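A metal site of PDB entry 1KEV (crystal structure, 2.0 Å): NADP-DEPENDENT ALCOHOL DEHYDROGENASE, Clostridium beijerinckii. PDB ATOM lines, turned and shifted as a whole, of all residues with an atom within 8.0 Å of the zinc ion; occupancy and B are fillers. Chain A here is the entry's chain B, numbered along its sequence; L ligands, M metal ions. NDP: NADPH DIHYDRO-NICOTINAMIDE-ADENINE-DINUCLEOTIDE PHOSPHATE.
O1N of the ligand is in hydrogen-bond range of OG1 of Thr 38, 3.0 Å away. N of Val 178 lies within hydrogen-bond range of O2N of the ligand.
OD1 of Asp 150 is in hydrogen-bond range of SG of Cys 85. OG1 of Thr 154 sits at hydrogen-bond distance from O of Asp 150 (2.8 Å). OG of Ser 39 sits close to SG of Cys 37, at 3.0 Å. The side-chain carboxylate (OD2) of Asp 40 lies within hydrogen-bond range of the backbone NH (N) of Cys 37. OE1 of Glu 60 is in salt-bridge range of NZ of Lys 346, at 3.1 Å. The backbone carbonyl oxygen (O) of Glu 60 lies within hydrogen-bond range of the backbone NH (N) of Ser 35, 3.2 Å away.
OD2 of Asp 150 binds the zinc ion. NE2 of His 59 binds the zinc ion (2.0 Å). SG of Cys 37 binds the zinc ion (2.4 Å). OE2 of Glu 60 is bound to the zinc ion (2.4 Å).
Merely in contact with the zinc ion: Ser 39 (3.9 Å). The nearest printed residue that does not touch the zinc ion is Met 151 (4.2 Å).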
ATOM      1  N   SER A  35     -12.990  31.726   0.051  1.00  0.00           N
ATOM      2  CA  SER A  35     -11.840  31.280  -0.724  1.00  0.00           C
ATOM      3  C   SER A  35     -11.874  31.810  -2.165  1.00  0.00           C
ATOM      4  O   SER A  35     -12.920  31.782  -2.829  1.00  0.00           O
ATOM      5  CB  SER A  35     -11.785  29.752  -0.748  1.00  0.00           C
ATOM      6  OG  SER A  35     -10.664  29.267  -1.477  1.00  0.00           O
ATOM      7  N   PRO A  36     -10.755  32.387  -2.627  1.00  0.00           N
ATOM      8  CA  PRO A  36     -10.665  32.929  -3.993  1.00  0.00           C
ATOM      9  C   PRO A  36     -10.584  31.780  -5.017  1.00  0.00           C
ATOM     10  O   PRO A  36     -10.013  30.728  -4.733  1.00  0.00           O
ATOM     11  CB  PRO A  36      -9.379  33.761  -3.942  1.00  0.00           C
ATOM     12  CG  PRO A  36      -8.531  33.008  -2.946  1.00  0.00           C
ATOM     13  CD  PRO A  36      -9.524  32.682  -1.856  1.00  0.00           C
ATOM     14  N   CYS A  37     -11.158  32.002  -6.193  1.00  0.00           N
ATOM     15  CA  CYS A  37     -11.166  30.980  -7.237  1.00  0.00           C
ATOM     16  C   CYS A  37     -10.486  31.405  -8.529  1.00  0.00           C
ATOM     17  O   CYS A  37     -10.392  32.603  -8.833  1.00  0.00           O
ATOM     18  CB  CYS A  37     -12.606  30.575  -7.543  1.00  0.00           C
ATOM     19  SG  CYS A  37     -12.812  29.306  -8.854  1.00  0.00           S
ATOM     20  N   THR A  38     -10.077  30.415  -9.317  1.00  0.00           N
ATOM     21  CA  THR A  38      -9.419  30.634 -10.603  1.00  0.00           C
ATOM     22  C   THR A  38     -10.293  31.434 -11.568  1.00  0.00           C
ATOM     23  O   THR A  38      -9.798  32.209 -12.388  1.00  0.00           O
ATOM     24  CB  THR A  38      -9.039  29.268 -11.227  1.00  0.00           C
ATOM     25  OG1 THR A  38      -8.284  28.505 -10.279  1.00  0.00           O
ATOM     26  CG2 THR A  38      -8.201  29.443 -12.489  1.00  0.00           C
ATOM     27  N   SER A  39     -11.608  31.258 -11.454  1.00  0.00           N
ATOM     28  CA  SER A  39     -12.572  31.954 -12.291  1.00  0.00           C
ATOM     29  C   SER A  39     -12.663  33.457 -11.973  1.00  0.00           C
ATOM     30  O   SER A  39     -12.909  34.271 -12.866  1.00  0.00           O
ATOM     31  CB  SER A  39     -13.948  31.291 -12.141  1.00  0.00           C
ATOM     32  OG  SER A  39     -14.265  31.121 -10.770  1.00  0.00           O
ATOM     33  N   ASP A  40     -12.434  33.817 -10.709  1.00  0.00           N
ATOM     34  CA  ASP A  40     -12.471  35.226 -10.281  1.00  0.00           C
ATOM     35  C   ASP A  40     -11.392  35.982 -11.045  1.00  0.00           C
ATOM     36  O   ASP A  40     -11.641  37.063 -11.584  1.00  0.00           O
ATOM     37  CB  ASP A  40     -12.199  35.357  -8.769  1.00  0.00           C
ATOM     38  CG  ASP A  40     -13.371  34.926  -7.899  1.00  0.00           C
ATOM     39  OD1 ASP A  40     -14.550  35.199  -8.255  1.00  0.00           O
ATOM     40  OD2 ASP A  40     -13.114  34.329  -6.835  1.00  0.00           O
ATOM     41  N   GLY A  58     -16.323  36.659  -5.832  1.00  0.00           N
ATOM     42  CA  GLY A  58     -16.356  35.471  -4.988  1.00  0.00           C
ATOM     43  C   GLY A  58     -17.605  34.600  -5.064  1.00  0.00           C
ATOM     44  O   GLY A  58     -18.715  35.108  -5.217  1.00  0.00           O
ATOM     45  N   HIS A  59     -17.419  33.283  -4.939  1.00  0.00           N
ATOM     46  CA  HIS A  59     -18.535  32.328  -4.976  1.00  0.00           C
ATOM     47  C   HIS A  59     -18.322  31.071  -4.115  1.00  0.00           C
ATOM     48  O   HIS A  59     -19.054  30.091  -4.251  1.00  0.00           O
ATOM     49  CB  HIS A  59     -18.926  31.943  -6.414  1.00  0.00           C
ATOM     50  CG  HIS A  59     -17.851  31.213  -7.177  1.00  0.00           C
ATOM     51  ND1 HIS A  59     -17.039  31.808  -8.113  1.00  0.00           N
ATOM     52  CD2 HIS A  59     -17.487  29.909  -7.143  1.00  0.00           C
ATOM     53  CE1 HIS A  59     -16.207  30.872  -8.605  1.00  0.00           C
ATOM     54  NE2 HIS A  59     -16.429  29.690  -8.056  1.00  0.00           N
ATOM     55  N   GLU A  60     -17.311  31.088  -3.256  1.00  0.00           N
ATOM     56  CA  GLU A  60     -17.014  29.952  -2.376  1.00  0.00           C
ATOM     57  C   GLU A  60     -17.020  30.412  -0.915  1.00  0.00           C
ATOM     58  O   GLU A  60     -16.101  31.121  -0.501  1.00  0.00           O
ATOM     59  CB  GLU A  60     -15.663  29.336  -2.735  1.00  0.00           C
ATOM     60  CG  GLU A  60     -15.634  28.702  -4.127  1.00  0.00           C
ATOM     61  CD  GLU A  60     -14.248  28.240  -4.541  1.00  0.00           C
ATOM     62  OE1 GLU A  60     -13.512  27.662  -3.714  1.00  0.00           O
ATOM     63  OE2 GLU A  60     -13.912  28.434  -5.718  1.00  0.00           O
ATOM     64  N   CYS A  85     -21.823  26.661  -4.570  1.00  0.00           N
ATOM     65  CA  CYS A  85     -21.605  27.753  -5.522  1.00  0.00           C
ATOM     66  C   CYS A  85     -22.701  27.874  -6.578  1.00  0.00           C
ATOM     67  O   CYS A  85     -22.899  28.940  -7.162  1.00  0.00           O
ATOM     68  CB  CYS A  85     -20.213  27.658  -6.180  1.00  0.00           C
ATOM     69  SG  CYS A  85     -19.948  26.258  -7.308  1.00  0.00           S
ATOM     70  N   TRP A 110     -25.436  29.366 -11.913  1.00  0.00           N
ATOM     71  CA  TRP A 110     -24.284  29.997 -11.310  1.00  0.00           C
ATOM     72  C   TRP A 110     -24.581  31.499 -11.206  1.00  0.00           C
ATOM     73  O   TRP A 110     -24.500  32.230 -12.191  1.00  0.00           O
ATOM     74  CB  TRP A 110     -23.044  29.739 -12.175  1.00  0.00           C
ATOM     75  CG  TRP A 110     -21.808  30.484 -11.780  1.00  0.00           C
ATOM     76  CD1 TRP A 110     -21.454  30.885 -10.526  1.00  0.00           C
ATOM     77  CD2 TRP A 110     -20.788  30.973 -12.656  1.00  0.00           C
ATOM     78  NE1 TRP A 110     -20.278  31.583 -10.564  1.00  0.00           N
ATOM     79  CE2 TRP A 110     -19.836  31.650 -11.860  1.00  0.00           C
ATOM     80  CE3 TRP A 110     -20.571  30.888 -14.045  1.00  0.00           C
ATOM     81  CZ2 TRP A 110     -18.696  32.256 -12.407  1.00  0.00           C
ATOM     82  CZ3 TRP A 110     -19.425  31.490 -14.579  1.00  0.00           C
ATOM     83  CH2 TRP A 110     -18.509  32.164 -13.755  1.00  0.00           C
ATOM     84  N   SER A 113     -21.082  36.346  -8.241  1.00  0.00           N
ATOM     85  CA  SER A 113     -20.047  36.944  -9.102  1.00  0.00           C
ATOM     86  C   SER A 113     -20.240  36.688 -10.599  1.00  0.00           C
ATOM     87  O   SER A 113     -19.280  36.470 -11.345  1.00  0.00           O
ATOM     88  CB  SER A 113     -18.632  36.573  -8.649  1.00  0.00           C
ATOM     89  OG  SER A 113     -18.415  35.163  -8.583  1.00  0.00           O
ATOM     90  N   THR A 149     -18.027  23.428  -1.392  1.00  0.00           N
ATOM     91  CA  THR A 149     -18.817  24.351  -2.214  1.00  0.00           C
ATOM     92  C   THR A 149     -18.541  24.359  -3.715  1.00  0.00           C
ATOM     93  O   THR A 149     -19.435  24.677  -4.510  1.00  0.00           O
ATOM     94  CB  THR A 149     -18.710  25.825  -1.681  1.00  0.00           C
ATOM     95  OG1 THR A 149     -17.362  26.276  -1.794  1.00  0.00           O
ATOM     96  CG2 THR A 149     -19.153  25.928  -0.230  1.00  0.00           C
ATOM     97  N   ASP A 150     -17.303  24.041  -4.107  1.00  0.00           N
ATOM     98  CA  ASP A 150     -16.942  24.061  -5.518  1.00  0.00           C
ATOM     99  C   ASP A 150     -15.935  23.002  -5.959  1.00  0.00           C
ATOM    100  O   ASP A 150     -16.197  22.261  -6.904  1.00  0.00           O
ATOM    101  CB  ASP A 150     -16.424  25.454  -5.860  1.00  0.00           C
ATOM    102  CG  ASP A 150     -16.171  25.657  -7.347  1.00  0.00           C
ATOM    103  OD1 ASP A 150     -16.705  24.903  -8.213  1.00  0.00           O
ATOM    104  OD2 ASP A 150     -15.426  26.620  -7.670  1.00  0.00           O
ATOM    105  N   MET A 151     -14.800  22.914  -5.274  1.00  0.00           N
ATOM    106  CA  MET A 151     -13.764  21.938  -5.640  1.00  0.00           C
ATOM    107  C   MET A 151     -14.240  20.461  -5.654  1.00  0.00           C
ATOM    108  O   MET A 151     -14.095  19.767  -6.663  1.00  0.00           O
ATOM    109  CB  MET A 151     -12.536  22.097  -4.727  1.00  0.00           C
ATOM    110  CG  MET A 151     -11.876  23.495  -4.761  1.00  0.00           C
ATOM    111  SD  MET A 151     -11.246  24.044  -6.382  1.00  0.00           S
ATOM    112  CE  MET A 151     -12.494  25.193  -6.877  1.00  0.00           C
ATOM    113  N   THR A 154     -17.267  19.738  -8.231  1.00  0.00           N
ATOM    114  CA  THR A 154     -16.829  19.797  -9.620  1.00  0.00           C
ATOM    115  C   THR A 154     -16.017  18.550 -10.011  1.00  0.00           C
ATOM    116  O   THR A 154     -16.360  17.862 -10.975  1.00  0.00           O
ATOM    117  CB  THR A 154     -16.061  21.102  -9.913  1.00  0.00           C
ATOM    118  OG1 THR A 154     -16.890  22.225  -9.644  1.00  0.00           O
ATOM    119  CG2 THR A 154     -15.595  21.163 -11.367  1.00  0.00           C
ATOM    120  N   VAL A 178      -9.211  21.138  -8.780  1.00  0.00           N
ATOM    121  CA  VAL A 178     -10.298  20.413  -9.448  1.00  0.00           C
ATOM    122  C   VAL A 178      -9.819  19.039  -9.947  1.00  0.00           C
ATOM    123  O   VAL A 178     -10.524  18.036  -9.781  1.00  0.00           O
ATOM    124  CB  VAL A 178     -10.880  21.245 -10.626  1.00  0.00           C
ATOM    125  CG1 VAL A 178     -11.850  20.425 -11.470  1.00  0.00           C
ATOM    126  CG2 VAL A 178     -11.586  22.462 -10.064  1.00  0.00           C
ATOM    127  N   CYS A 295     -20.851  22.036 -12.430  1.00  0.00           N
ATOM    128  CA  CYS A 295     -21.116  21.261 -11.227  1.00  0.00           C
ATOM    129  C   CYS A 295     -22.547  21.447 -10.717  1.00  0.00           C
ATOM    130  O   CYS A 295     -23.123  22.527 -10.852  1.00  0.00           O
ATOM    131  CB  CYS A 295     -20.128  21.622 -10.111  1.00  0.00           C
ATOM    132  SG  CYS A 295     -20.239  23.327  -9.460  1.00  0.00           S
ATOM    133  N   MET A 337      -3.690  34.369  -5.741  1.00  0.00           N
ATOM    134  CA  MET A 337      -4.195  33.532  -6.835  1.00  0.00           C
ATOM    135  C   MET A 337      -3.756  34.048  -8.194  1.00  0.00           C
ATOM    136  O   MET A 337      -3.631  33.270  -9.148  1.00  0.00           O
ATOM    137  CB  MET A 337      -5.725  33.447  -6.797  1.00  0.00           C
ATOM    138  CG  MET A 337      -6.299  32.497  -5.733  1.00  0.00           C
ATOM    139  SD  MET A 337      -5.941  30.743  -6.013  1.00  0.00           S
ATOM    140  CE  MET A 337      -7.238  30.298  -7.126  1.00  0.00           C
ATOM    141  N   LYS A 346      -4.860  25.968  -2.737  1.00  0.00           N
ATOM    142  CA  LYS A 346      -6.017  26.810  -2.411  1.00  0.00           C
ATOM    143  C   LYS A 346      -5.739  27.595  -1.133  1.00  0.00           C
ATOM    144  O   LYS A 346      -4.954  27.150  -0.280  1.00  0.00           O
ATOM    145  CB  LYS A 346      -7.279  25.952  -2.230  1.00  0.00           C
ATOM    146  CG  LYS A 346      -7.846  25.354  -3.523  1.00  0.00           C
ATOM    147  CD  LYS A 346      -8.506  26.393  -4.407  1.00  0.00           C
ATOM    148  CE  LYS A 346      -9.874  26.810  -3.857  1.00  0.00           C
ATOM    149  NZ  LYS A 346     -10.651  27.633  -4.827  1.00  0.00           N
HETATM  150  PA  NDP L   1      -5.105  25.033 -12.157  1.00  0.00           P
HETATM  151  O1A NDP L   1      -5.138  26.400 -12.773  1.00  0.00           O
HETATM  152  O2A NDP L   1      -4.454  24.908 -10.811  1.00  0.00           O
HETATM  153  O5B NDP L   1      -4.213  24.059 -13.168  1.00  0.00           O
HETATM  154  C5B NDP L   1      -4.458  22.637 -13.297  1.00  0.00           C
HETATM  155  C4B NDP L   1      -3.438  21.959 -14.213  1.00  0.00           C
HETATM  156  O4B NDP L   1      -3.355  22.628 -15.503  1.00  0.00           O
HETATM  157  C3B NDP L   1      -2.031  21.920 -13.588  1.00  0.00           C
HETATM  158  O3B NDP L   1      -1.754  20.720 -12.866  1.00  0.00           O
HETATM  159  C2B NDP L   1      -1.143  21.926 -14.813  1.00  0.00           C
HETATM  160  O2B NDP L   1       0.294  22.022 -14.814  1.00  0.00           O
HETATM  161  C1B NDP L   1      -2.039  22.309 -15.969  1.00  0.00           C
HETATM  162  N9A NDP L   1      -1.623  22.244 -17.393  1.00  0.00           N
HETATM  163  C8A NDP L   1      -1.208  23.296 -18.131  1.00  0.00           C
HETATM  164  N7A NDP L   1      -0.913  22.923 -19.378  1.00  0.00           N
HETATM  165  C5A NDP L   1      -1.152  21.612 -19.370  1.00  0.00           C
HETATM  166  C6A NDP L   1      -0.979  20.784 -20.480  1.00  0.00           C
HETATM  167  N6A NDP L   1      -0.546  21.293 -21.629  1.00  0.00           N
HETATM  168  N1A NDP L   1      -1.274  19.479 -20.295  1.00  0.00           N
HETATM  169  C2A NDP L   1      -1.700  19.024 -19.110  1.00  0.00           C
HETATM  170  N3A NDP L   1      -1.856  19.822 -18.054  1.00  0.00           N
HETATM  171  C4A NDP L   1      -1.593  21.142 -18.161  1.00  0.00           C
HETATM  172  O3  NDP L   1      -6.600  24.394 -12.150  1.00  0.00           O
HETATM  173  PN  NDP L   1      -7.964  24.391 -11.305  1.00  0.00           P
HETATM  174  O1N NDP L   1      -8.065  25.519 -10.318  1.00  0.00           O
HETATM  175  O2N NDP L   1      -8.137  23.020 -10.677  1.00  0.00           O
HETATM  176  O5D NDP L   1      -9.159  24.668 -12.413  1.00  0.00           O
HETATM  177  C5D NDP L   1      -9.544  23.710 -13.482  1.00  0.00           C
HETATM  178  C4D NDP L   1     -10.686  24.195 -14.491  1.00  0.00           C
HETATM  179  O4D NDP L   1     -12.079  23.944 -14.114  1.00  0.00           O
HETATM  180  C3D NDP L   1     -10.486  25.743 -14.700  1.00  0.00           C
HETATM  181  O3D NDP L   1     -10.862  26.259 -15.983  1.00  0.00           O
HETATM  182  C2D NDP L   1     -11.631  26.254 -13.809  1.00  0.00           C
HETATM  183  O2D NDP L   1     -12.256  27.579 -14.045  1.00  0.00           O
HETATM  184  C1D NDP L   1     -12.736  25.169 -13.955  1.00  0.00           C
HETATM  185  N1N NDP L   1     -13.748  25.307 -12.810  1.00  0.00           N
HETATM  186  C2N NDP L   1     -15.042  25.992 -12.896  1.00  0.00           C
HETATM  187  C3N NDP L   1     -15.701  26.331 -11.698  1.00  0.00           C
HETATM  188  C7N NDP L   1     -17.103  26.978 -11.709  1.00  0.00           C
HETATM  189  O7N NDP L   1     -17.989  26.840 -10.847  1.00  0.00           O
HETATM  190  N7N NDP L   1     -17.282  27.789 -12.750  1.00  0.00           N
HETATM  191  C4N NDP L   1     -15.058  26.023 -10.493  1.00  0.00           C
HETATM  192  C5N NDP L   1     -13.837  25.329 -10.422  1.00  0.00           C
HETATM  193  C6N NDP L   1     -13.164  24.964 -11.562  1.00  0.00           C
HETATM  194  P2B NDP L   1       1.143  22.832 -13.704  1.00  0.00           P
HETATM  195  O1X NDP L   1       2.381  23.191 -14.431  1.00  0.00           O
HETATM  196  O2X NDP L   1       1.322  21.807 -12.636  1.00  0.00           O
HETATM  197  O3X NDP L   1       0.334  24.019 -13.323  1.00  0.00           O
HETATM  198 ZN    ZN M   1     -14.878  28.459  -7.947  1.00  0.00          ZN
